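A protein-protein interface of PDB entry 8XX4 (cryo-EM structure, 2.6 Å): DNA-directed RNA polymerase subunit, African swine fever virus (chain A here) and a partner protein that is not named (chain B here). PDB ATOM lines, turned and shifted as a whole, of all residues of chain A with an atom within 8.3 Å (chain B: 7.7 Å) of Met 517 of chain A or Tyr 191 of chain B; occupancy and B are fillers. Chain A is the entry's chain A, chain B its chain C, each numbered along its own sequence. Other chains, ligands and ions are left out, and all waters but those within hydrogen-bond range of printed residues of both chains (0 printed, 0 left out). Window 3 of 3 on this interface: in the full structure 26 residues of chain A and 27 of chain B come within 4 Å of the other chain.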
ATOM      1  N   ARG A 512      13.137   5.976 -21.507  1.00  0.00           N
ATOM      2  CA  ARG A 512      13.226   5.883 -20.059  1.00  0.00           C
ATOM      3  C   ARG A 512      14.080   7.019 -19.517  1.00  0.00           C
ATOM      4  O   ARG A 512      14.987   7.515 -20.185  1.00  0.00           O
ATOM      5  CB  ARG A 512      13.793   4.531 -19.636  1.00  0.00           C
ATOM      6  CG  ARG A 512      15.285   4.417 -19.753  1.00  0.00           C
ATOM      7  CD  ARG A 512      15.752   3.011 -19.478  1.00  0.00           C
ATOM      8  NE  ARG A 512      17.035   2.757 -20.116  1.00  0.00           N
ATOM      9  CZ  ARG A 512      17.866   1.786 -19.770  1.00  0.00           C
ATOM     10  NH1 ARG A 512      17.575   0.945 -18.793  1.00  0.00           N
ATOM     11  NH2 ARG A 512      19.016   1.655 -20.423  1.00  0.00           N
ATOM     12  N   ASN A 514      16.091   7.278 -16.697  1.00  0.00           N
ATOM     13  CA  ASN A 514      17.391   6.984 -16.122  1.00  0.00           C
ATOM     14  C   ASN A 514      17.900   5.647 -16.631  1.00  0.00           C
ATOM     15  O   ASN A 514      17.149   4.670 -16.697  1.00  0.00           O
ATOM     16  CB  ASN A 514      17.320   6.949 -14.595  1.00  0.00           C
ATOM     17  CG  ASN A 514      17.538   8.302 -13.969  1.00  0.00           C
ATOM     18  OD1 ASN A 514      17.138   9.325 -14.517  1.00  0.00           O
ATOM     19  ND2 ASN A 514      18.174   8.317 -12.807  1.00  0.00           N
ATOM     20  N   THR A 515      19.171   5.609 -16.980  1.00  0.00           N
ATOM     21  CA  THR A 515      19.905   4.390 -17.256  1.00  0.00           C
ATOM     22  C   THR A 515      20.824   4.081 -16.086  1.00  0.00           C
ATOM     23  O   THR A 515      21.008   4.912 -15.190  1.00  0.00           O
ATOM     24  CB  THR A 515      20.719   4.533 -18.548  1.00  0.00           C
ATOM     25  OG1 THR A 515      21.879   5.332 -18.301  1.00  0.00           O
ATOM     26  CG2 THR A 515      19.892   5.187 -19.621  1.00  0.00           C
ATOM     27  N   PRO A 516      21.406   2.882 -16.042  1.00  0.00           N
ATOM     28  CA  PRO A 516      22.415   2.610 -15.007  1.00  0.00           C
ATOM     29  C   PRO A 516      23.608   3.551 -15.057  1.00  0.00           C
ATOM     30  O   PRO A 516      24.329   3.660 -14.060  1.00  0.00           O
ATOM     31  CB  PRO A 516      22.828   1.158 -15.286  1.00  0.00           C
ATOM     32  CG  PRO A 516      22.151   0.775 -16.571  1.00  0.00           C
ATOM     33  CD  PRO A 516      20.962   1.643 -16.695  1.00  0.00           C
ATOM     34  N   MET A 517      23.838   4.232 -16.177  1.00  0.00           N
ATOM     35  CA  MET A 517      24.906   5.216 -16.282  1.00  0.00           C
ATOM     36  C   MET A 517      24.501   6.593 -15.774  1.00  0.00           C
ATOM     37  O   MET A 517      25.346   7.493 -15.742  1.00  0.00           O
ATOM     38  CB  MET A 517      25.377   5.333 -17.736  1.00  0.00           C
ATOM     39  CG  MET A 517      26.329   4.244 -18.277  1.00  0.00           C
ATOM     40  SD  MET A 517      27.875   3.833 -17.424  1.00  0.00           S
ATOM     41  CE  MET A 517      27.356   3.036 -15.907  1.00  0.00           C
ATOM     42  N   GLY A 518      23.243   6.779 -15.376  1.00  0.00           N
ATOM     43  CA  GLY A 518      22.740   8.070 -14.954  1.00  0.00           C
ATOM     44  C   GLY A 518      21.525   8.474 -15.775  1.00  0.00           C
ATOM     45  O   GLY A 518      20.692   7.642 -16.126  1.00  0.00           O
ATOM     46  N   LYS A 519      21.439   9.769 -16.068  1.00  0.00           N
ATOM     47  CA  LYS A 519      20.350  10.263 -16.896  1.00  0.00           C
ATOM     48  C   LYS A 519      20.481   9.733 -18.316  1.00  0.00           C
ATOM     49  O   LYS A 519      21.584   9.601 -18.852  1.00  0.00           O
ATOM     50  CB  LYS A 519      20.337  11.786 -16.902  1.00  0.00           C
ATOM     51  CG  LYS A 519      19.194  12.393 -16.127  1.00  0.00           C
ATOM     52  CD  LYS A 519      19.129  13.890 -16.345  1.00  0.00           C
ATOM     53  CE  LYS A 519      18.905  14.223 -17.808  1.00  0.00           C
ATOM     54  NZ  LYS A 519      17.482  14.068 -18.209  1.00  0.00           N
ATOM     55  N   ASN A 520      19.339   9.430 -18.929  1.00  0.00           N
ATOM     56  CA  ASN A 520      19.301   8.877 -20.280  1.00  0.00           C
ATOM     57  C   ASN A 520      19.460  10.021 -21.273  1.00  0.00           C
ATOM     58  O   ASN A 520      18.501  10.531 -21.855  1.00  0.00           O
ATOM     59  CB  ASN A 520      18.006   8.110 -20.500  1.00  0.00           C
ATOM     60  CG  ASN A 520      18.040   7.254 -21.738  1.00  0.00           C
ATOM     61  OD1 ASN A 520      19.095   7.017 -22.316  1.00  0.00           O
ATOM     62  ND2 ASN A 520      16.881   6.766 -22.143  1.00  0.00           N
ATOM     63  N   VAL A 521      20.712  10.430 -21.469  1.00  0.00           N
ATOM     64  CA  VAL A 521      21.046  11.533 -22.354  1.00  0.00           C
ATOM     65  C   VAL A 521      22.094  11.069 -23.352  1.00  0.00           C
ATOM     66  O   VAL A 521      22.857  10.136 -23.103  1.00  0.00           O
ATOM     67  CB  VAL A 521      21.556  12.771 -21.592  1.00  0.00           C
ATOM     68  CG1 VAL A 521      20.397  13.543 -21.005  1.00  0.00           C
ATOM     69  CG2 VAL A 521      22.533  12.362 -20.512  1.00  0.00           C
ATOM     70  N   GLU A 726      16.536  -2.408 -13.996  1.00  0.00           N
ATOM     71  CA  GLU A 726      17.239  -1.510 -14.897  1.00  0.00           C
ATOM     72  C   GLU A 726      18.175  -2.234 -15.852  1.00  0.00           C
ATOM     73  O   GLU A 726      18.538  -1.664 -16.884  1.00  0.00           O
ATOM     74  CB  GLU A 726      18.037  -0.480 -14.098  1.00  0.00           C
ATOM     75  CG  GLU A 726      17.198   0.630 -13.508  1.00  0.00           C
ATOM     76  CD  GLU A 726      17.746   2.006 -13.831  1.00  0.00           C
ATOM     77  OE1 GLU A 726      18.862   2.324 -13.371  1.00  0.00           O
ATOM     78  OE2 GLU A 726      17.061   2.768 -14.545  1.00  0.00           O
ATOM     79  N   THR A 727      18.574  -3.466 -15.540  1.00  0.00           N
ATOM     80  CA  THR A 727      19.550  -4.174 -16.350  1.00  0.00           C
ATOM     81  C   THR A 727      19.114  -5.572 -16.764  1.00  0.00           C
ATOM     82  O   THR A 727      19.832  -6.217 -17.532  1.00  0.00           O
ATOM     83  CB  THR A 727      20.890  -4.281 -15.610  1.00  0.00           C
ATOM     84  OG1 THR A 727      20.677  -4.849 -14.313  1.00  0.00           O
ATOM     85  CG2 THR A 727      21.527  -2.917 -15.455  1.00  0.00           C
ATOM     86  N   ILE B 188      38.893   6.442 -20.855  1.00  0.00           N
ATOM     87  CA  ILE B 188      37.617   6.268 -20.176  1.00  0.00           C
ATOM     88  C   ILE B 188      37.840   5.333 -18.999  1.00  0.00           C
ATOM     89  O   ILE B 188      38.423   4.257 -19.157  1.00  0.00           O
ATOM     90  CB  ILE B 188      36.532   5.714 -21.117  1.00  0.00           C
ATOM     91  CG1 ILE B 188      36.460   6.539 -22.396  1.00  0.00           C
ATOM     92  CG2 ILE B 188      35.181   5.716 -20.427  1.00  0.00           C
ATOM     93  CD1 ILE B 188      35.299   6.177 -23.275  1.00  0.00           C
ATOM     94  N   GLU B 189      37.395   5.755 -17.821  1.00  0.00           N
ATOM     95  CA  GLU B 189      37.554   4.941 -16.628  1.00  0.00           C
ATOM     96  C   GLU B 189      36.639   3.726 -16.693  1.00  0.00           C
ATOM     97  O   GLU B 189      35.571   3.757 -17.307  1.00  0.00           O
ATOM     98  CB  GLU B 189      37.255   5.754 -15.365  1.00  0.00           C
ATOM     99  CG  GLU B 189      37.594   7.247 -15.429  1.00  0.00           C
ATOM    100  CD  GLU B 189      36.623   8.060 -16.276  1.00  0.00           C
ATOM    101  OE1 GLU B 189      35.403   7.806 -16.197  1.00  0.00           O
ATOM    102  OE2 GLU B 189      37.082   8.948 -17.023  1.00  0.00           O
ATOM    103  N   GLN B 190      37.065   2.648 -16.046  1.00  0.00           N
ATOM    104  CA  GLN B 190      36.354   1.381 -16.091  1.00  0.00           C
ATOM    105  C   GLN B 190      35.917   0.958 -14.697  1.00  0.00           C
ATOM    106  O   GLN B 190      36.627   1.187 -13.714  1.00  0.00           O
ATOM    107  CB  GLN B 190      37.219   0.285 -16.704  1.00  0.00           C
ATOM    108  CG  GLN B 190      37.624   0.539 -18.130  1.00  0.00           C
ATOM    109  CD  GLN B 190      37.480  -0.689 -18.990  1.00  0.00           C
ATOM    110  OE1 GLN B 190      36.460  -1.373 -18.944  1.00  0.00           O
ATOM    111  NE2 GLN B 190      38.503  -0.982 -19.780  1.00  0.00           N
ATOM    112  N   TYR B 191      34.745   0.337 -14.624  1.00  0.00           N
ATOM    113  CA  TYR B 191      34.267  -0.252 -13.390  1.00  0.00           C
ATOM    114  C   TYR B 191      34.968  -1.581 -13.127  1.00  0.00           C
ATOM    115  O   TYR B 191      35.510  -2.202 -14.042  1.00  0.00           O
ATOM    116  CB  TYR B 191      32.763  -0.487 -13.460  1.00  0.00           C
ATOM    117  CG  TYR B 191      31.921   0.749 -13.315  1.00  0.00           C
ATOM    118  CD1 TYR B 191      32.037   1.564 -12.201  1.00  0.00           C
ATOM    119  CD2 TYR B 191      30.998   1.094 -14.286  1.00  0.00           C
ATOM    120  CE1 TYR B 191      31.265   2.692 -12.067  1.00  0.00           C
ATOM    121  CE2 TYR B 191      30.225   2.216 -14.160  1.00  0.00           C
ATOM    122  CZ  TYR B 191      30.359   3.013 -13.049  1.00  0.00           C
ATOM    123  OH  TYR B 191      29.582   4.140 -12.925  1.00  0.00           O
ATOM    124  N   PRO B 192      34.975  -2.034 -11.878  1.00  0.00           N
ATOM    125  CA  PRO B 192      35.353  -3.432 -11.579  1.00  0.00           C
ATOM    126  C   PRO B 192      34.185  -4.388 -11.819  1.00  0.00           C
ATOM    127  O   PRO B 192      33.408  -4.734 -10.932  1.00  0.00           O
ATOM    128  CB  PRO B 192      35.757  -3.362 -10.106  1.00  0.00           C
ATOM    129  CG  PRO B 192      34.960  -2.242  -9.558  1.00  0.00           C
ATOM    130  CD  PRO B 192      34.822  -1.230 -10.654  1.00  0.00           C
ATOM    131  N   THR B 193      34.047  -4.827 -13.071  1.00  0.00           N
ATOM    132  CA  THR B 193      32.900  -5.625 -13.494  1.00  0.00           C
ATOM    133  C   THR B 193      32.893  -7.034 -12.921  1.00  0.00           C
ATOM    134  O   THR B 193      31.985  -7.803 -13.252  1.00  0.00           O
ATOM    135  CB  THR B 193      32.842  -5.707 -15.017  1.00  0.00           C
ATOM    136  OG1 THR B 193      34.170  -5.833 -15.543  1.00  0.00           O
ATOM    137  CG2 THR B 193      32.186  -4.466 -15.584  1.00  0.00           C
ATOM    138  N   ASP B 194      33.872  -7.405 -12.097  1.00  0.00           N
ATOM    139  CA  ASP B 194      33.790  -8.673 -11.387  1.00  0.00           C
ATOM    140  C   ASP B 194      32.718  -8.658 -10.305  1.00  0.00           C
ATOM    141  O   ASP B 194      32.360  -9.724  -9.799  1.00  0.00           O
ATOM    142  CB  ASP B 194      35.146  -9.023 -10.776  1.00  0.00           C
ATOM    143  CG  ASP B 194      35.769  -7.858 -10.037  1.00  0.00           C
ATOM    144  OD1 ASP B 194      35.223  -7.456  -8.988  1.00  0.00           O
ATOM    145  OD2 ASP B 194      36.806  -7.343 -10.503  1.00  0.00           O
ATOM    146  N   LYS B 195      32.203  -7.487  -9.949  1.00  0.00           N
ATOM    147  CA  LYS B 195      31.149  -7.366  -8.956  1.00  0.00           C
ATOM    148  C   LYS B 195      29.786  -7.577  -9.601  1.00  0.00           C
ATOM    149  O   LYS B 195      29.594  -7.322 -10.791  1.00  0.00           O
ATOM    150  CB  LYS B 195      31.197  -5.994  -8.282  1.00  0.00           C
ATOM    151  CG  LYS B 195      32.525  -5.675  -7.621  1.00  0.00           C
ATOM    152  CD  LYS B 195      32.730  -4.176  -7.505  1.00  0.00           C
ATOM    153  CE  LYS B 195      33.071  -3.766  -6.083  1.00  0.00           C
ATOM    154  NZ  LYS B 195      33.580  -2.370  -6.015  1.00  0.00           N
ATOM    155  N   GLU B 197      27.171  -5.882  -9.148  1.00  0.00           N
ATOM    156  CA  GLU B 197      26.486  -4.632  -9.438  1.00  0.00           C
ATOM    157  C   GLU B 197      26.969  -3.974 -10.720  1.00  0.00           C
ATOM    158  O   GLU B 197      26.398  -2.957 -11.125  1.00  0.00           O
ATOM    159  CB  GLU B 197      26.647  -3.660  -8.269  1.00  0.00           C
ATOM    160  CG  GLU B 197      28.082  -3.281  -7.971  1.00  0.00           C
ATOM    161  CD  GLU B 197      28.607  -3.950  -6.721  1.00  0.00           C
ATOM    162  OE1 GLU B 197      27.887  -4.800  -6.158  1.00  0.00           O
ATOM    163  OE2 GLU B 197      29.736  -3.624  -6.299  1.00  0.00           O
ATOM    164  N   TYR B 198      27.999  -4.519 -11.364  1.00  0.00           N
ATOM    165  CA  TYR B 198      28.501  -3.971 -12.614  1.00  0.00           C
ATOM    166  C   TYR B 198      28.595  -4.994 -13.734  1.00  0.00           C
ATOM    167  O   TYR B 198      28.952  -4.620 -14.853  1.00  0.00           O
ATOM    168  CB  TYR B 198      29.885  -3.337 -12.411  1.00  0.00           C
ATOM    169  CG  TYR B 198      29.908  -2.210 -11.411  1.00  0.00           C
ATOM    170  CD1 TYR B 198      29.007  -1.160 -11.499  1.00  0.00           C
ATOM    171  CD2 TYR B 198      30.834  -2.192 -10.380  1.00  0.00           C
ATOM    172  CE1 TYR B 198      29.026  -0.130 -10.588  1.00  0.00           C
ATOM    173  CE2 TYR B 198      30.860  -1.165  -9.464  1.00  0.00           C
ATOM    174  CZ  TYR B 198      29.955  -0.137  -9.573  1.00  0.00           C
ATOM    175  OH  TYR B 198      29.977   0.891  -8.661  1.00  0.00           O
ATOM    176  N   MET B 199      28.288  -6.265 -13.476  1.00  0.00           N
ATOM    177  CA  MET B 199      28.511  -7.293 -14.483  1.00  0.00           C
ATOM    178  C   MET B 199      27.536  -7.197 -15.647  1.00  0.00           C
ATOM    179  O   MET B 199      27.803  -7.768 -16.708  1.00  0.00           O
ATOM    180  CB  MET B 199      28.438  -8.679 -13.846  1.00  0.00           C
ATOM    181  CG  MET B 199      27.150  -8.972 -13.116  1.00  0.00           C
ATOM    182  SD  MET B 199      27.013 -10.714 -12.687  1.00  0.00           S
ATOM    183  CE  MET B 199      25.248 -10.953 -12.801  1.00  0.00           C
ATOM    184  N   LEU B 201      26.857  -4.332 -17.076  1.00  0.00           N
ATOM    185  CA  LEU B 201      27.273  -3.148 -17.806  1.00  0.00           C
ATOM    186  C   LEU B 201      28.553  -3.433 -18.579  1.00  0.00           C
ATOM    187  O   LEU B 201      29.248  -4.419 -18.327  1.00  0.00           O
ATOM    188  CB  LEU B 201      27.486  -1.970 -16.855  1.00  0.00           C
ATOM    189  CG  LEU B 201      26.380  -1.734 -15.830  1.00  0.00           C
ATOM    190  CD1 LEU B 201      26.747  -0.593 -14.906  1.00  0.00           C
ATOM    191  CD2 LEU B 201      25.076  -1.448 -16.534  1.00  0.00           C
ATOM    192  N   SER B 202      28.857  -2.553 -19.533  1.00  0.00           N
ATOM    193  CA  SER B 202      30.061  -2.733 -20.335  1.00  0.00           C
ATOM    194  C   SER B 202      31.310  -2.648 -19.474  1.00  0.00           C
ATOM    195  O   SER B 202      32.270  -3.398 -19.682  1.00  0.00           O
ATOM    196  CB  SER B 202      30.116  -1.692 -21.448  1.00  0.00           C
ATOM    197  OG  SER B 202      30.378  -0.408 -20.926  1.00  0.00           O
ATOM    198  N   GLY B 203      31.313  -1.747 -18.501  1.00  0.00           N
ATOM    199  CA  GLY B 203      32.454  -1.581 -17.630  1.00  0.00           C
ATOM    200  C   GLY B 203      32.940  -0.153 -17.642  1.00  0.00           C
ATOM    201  O   GLY B 203      33.430   0.354 -16.633  1.00  0.00           O
ATOM    202  N   TYR B 204      32.805   0.504 -18.787  1.00  0.00           N
ATOM    203  CA  TYR B 204      33.174   1.904 -18.895  1.00  0.00           C
ATOM    204  C   TYR B 204      32.266   2.755 -18.023  1.00  0.00           C
ATOM    205  O   TYR B 204      31.066   2.499 -17.912  1.00  0.00           O
ATOM    206  CB  TYR B 204      33.094   2.359 -20.346  1.00  0.00           C
ATOM    207  CG  TYR B 204      34.217   1.839 -21.199  1.00  0.00           C
ATOM    208  CD1 TYR B 204      35.536   2.060 -20.848  1.00  0.00           C
ATOM    209  CD2 TYR B 204      33.959   1.122 -22.350  1.00  0.00           C
ATOM    210  CE1 TYR B 204      36.562   1.587 -21.621  1.00  0.00           C
ATOM    211  CE2 TYR B 204      34.979   0.649 -23.131  1.00  0.00           C
ATOM    212  CZ  TYR B 204      36.279   0.882 -22.762  1.00  0.00           C
ATOM    213  OH  TYR B 204      37.303   0.403 -23.537  1.00  0.00           O
ATOM    214  N   LYS B 205      32.847   3.773 -17.397  1.00  0.00           N
ATOM    215  CA  LYS B 205      32.087   4.631 -16.504  1.00  0.00           C
ATOM    216  C   LYS B 205      31.283   5.691 -17.237  1.00  0.00           C
ATOM    217  O   LYS B 205      30.474   6.375 -16.605  1.00  0.00           O
ATOM    218  CB  LYS B 205      33.028   5.295 -15.502  1.00  0.00           C
ATOM    219  CG  LYS B 205      33.608   4.329 -14.489  1.00  0.00           C
ATOM    220  CD  LYS B 205      33.977   5.031 -13.202  1.00  0.00           C
ATOM    221  CE  LYS B 205      34.684   4.092 -12.252  1.00  0.00           C
ATOM    222  NZ  LYS B 205      36.124   4.422 -12.125  1.00  0.00           N
ATOM    223  N   GLN B 206      31.476   5.843 -18.543  1.00  0.00           N
ATOM    224  CA  GLN B 206      30.741   6.807 -19.345  1.00  0.00           C
ATOM    225  C   GLN B 206      29.881   6.088 -20.370  1.00  0.00           C
ATOM    226  O   GLN B 206      30.324   5.123 -20.998  1.00  0.00           O
ATOM    227  CB  GLN B 206      31.687   7.766 -20.063  1.00  0.00           C
ATOM    228  CG  GLN B 206      32.494   8.648 -19.149  1.00  0.00           C
ATOM    229  CD  GLN B 206      33.593   9.374 -19.883  1.00  0.00           C
ATOM    230  OE1 GLN B 206      33.371   9.941 -20.950  1.00  0.00           O
ATOM    231  NE2 GLN B 206      34.791   9.360 -19.315  1.00  0.00           N
ATOM    232  N   SER B 207      28.652   6.562 -20.539  1.00  0.00           N
ATOM    233  CA  SER B 207      27.791   6.027 -21.581  1.00  0.00           C
ATOM    234  C   SER B 207      28.364   6.348 -22.953  1.00  0.00           C
ATOM    235  O   SER B 207      28.857   7.450 -23.196  1.00  0.00           O
ATOM    236  CB  SER B 207      26.385   6.606 -21.451  1.00  0.00           C
ATOM    237  OG  SER B 207      25.686   6.520 -22.675  1.00  0.00           O
ATOM    238  N   SER B 208      28.304   5.369 -23.857  1.00  0.00           N
ATOM    239  CA  SER B 208      28.814   5.578 -25.206  1.00  0.00           C
ATOM    240  C   SER B 208      28.020   6.624 -25.966  1.00  0.00           C
ATOM    241  O   SER B 208      28.532   7.186 -26.939  1.00  0.00           O
ATOM    242  CB  SER B 208      28.815   4.263 -25.979  1.00  0.00           C
ATOM    243  OG  SER B 208      27.602   3.563 -25.794  1.00  0.00           O
ATOM    244  N   THR B 210      27.415   9.485 -24.888  1.00  0.00           N
ATOM    245  CA  THR B 210      28.005  10.771 -24.559  1.00  0.00           C
ATOM    246  C   THR B 210      29.524  10.792 -24.619  1.00  0.00           C
ATOM    247  O   THR B 210      30.097  11.866 -24.820  1.00  0.00           O
ATOM    248  CB  THR B 210      27.578  11.224 -23.153  1.00  0.00           C
ATOM    249  OG1 THR B 210      28.173  10.367 -22.174  1.00  0.00           O
ATOM    250  CG2 THR B 210      26.074  11.181 -23.006  1.00  0.00           C
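The backbone carbonyl oxygen (O) of Tyr 204 of chain B lies close to the side-chain sulfur (SD) of Met 517 of chain A (3.5 Å).
O of Lys 205 of chain B lies close to SD of Met 517 of chain A (3.7 Å).
N of Tyr 204 of chain B is in hydrogen-bond range of OG of Ser 202 of chain B (3.4 Å).
The backbone NH (N) of Lys 205 of chain B is in hydrogen-bond range of the backbone carbonyl oxygen (O) of Glu 189 of chain B, 2.7 Å away.
The backbone carbonyl oxygen (O) of Gly 203 of chain B sits at hydrogen-bond distance from the backbone NH (N) of Tyr 191 of chain B, at 2.4 Å.
N of Met 517 of chain A sits close to OG1 of Thr 515 of chain A (3.1 Å).
O of Ser 207 of chain B lies within hydrogen-bond range of OG1 of Thr 210 of chain B (3.2 Å).
Among the printed residues, pairs that only touch across the chains: Pro 516 of chain A with Leu 201 of chain B (3.7 Å), Met 517 of chain A with Tyr 191 of chain B (3.5 Å), Met 517 of chain A with Leu 201 of chain B (3.8 Å), Met 517 of chain A with Ser 207 of chain B (3.96 Å), Val 521 of chain A with Thr 210 of chain B (3.4 Å) and Thr 727 of chain A with Leu 201 of chain B (3.99 Å).
Met 517 of chain A touches five residues of chain B.
Of the printed residues of chain B, Val 521 of chain A touches Thr 210 (3.4 Å).
Of the printed residues of chain B, Thr 727 of chain A touches Leu 201 (3.99 Å).
Pro 192 of chain B touches none of the printed residues of chain A.
Glu 197 of chain B touches none of the printed residues of chain A.
Of the printed residues of chain A, Tyr 204 of chain B touches Met 517.
Printed residues of chain A within 4 Å of Ser 207 of chain B: Met 517 (3.96 Å).
Printed residues of chain A within 4 Å of Thr 210 of chain B: Val 521.
The nearest residue of chain A that does not touch Tyr 191 of chain B is Pro 516 of chain A (5.4 Å).
Printed residues of chain B that touch a printed residue of chain A: Tyr 191, Leu 201, Tyr 204, Lys 205, Ser 207 and Thr 210.
Hydrophobic or aromatic side chains of chain B that line the printed part of chain A: Tyr 191 and Leu 201.
Of the 11 printed residues of chain A, 4 touch a printed residue of chain B.
Printed residues of chain A that touch a printed residue of chain B: Pro 516, Met 517, Val 521 and Thr 727.
Hydrophobic or aromatic side chains of chain A that line the printed part of chain B: Pro 516 and Met 517.
Along chain A the printed residues that touch a printed residue of chain B span positions 516 to 727.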
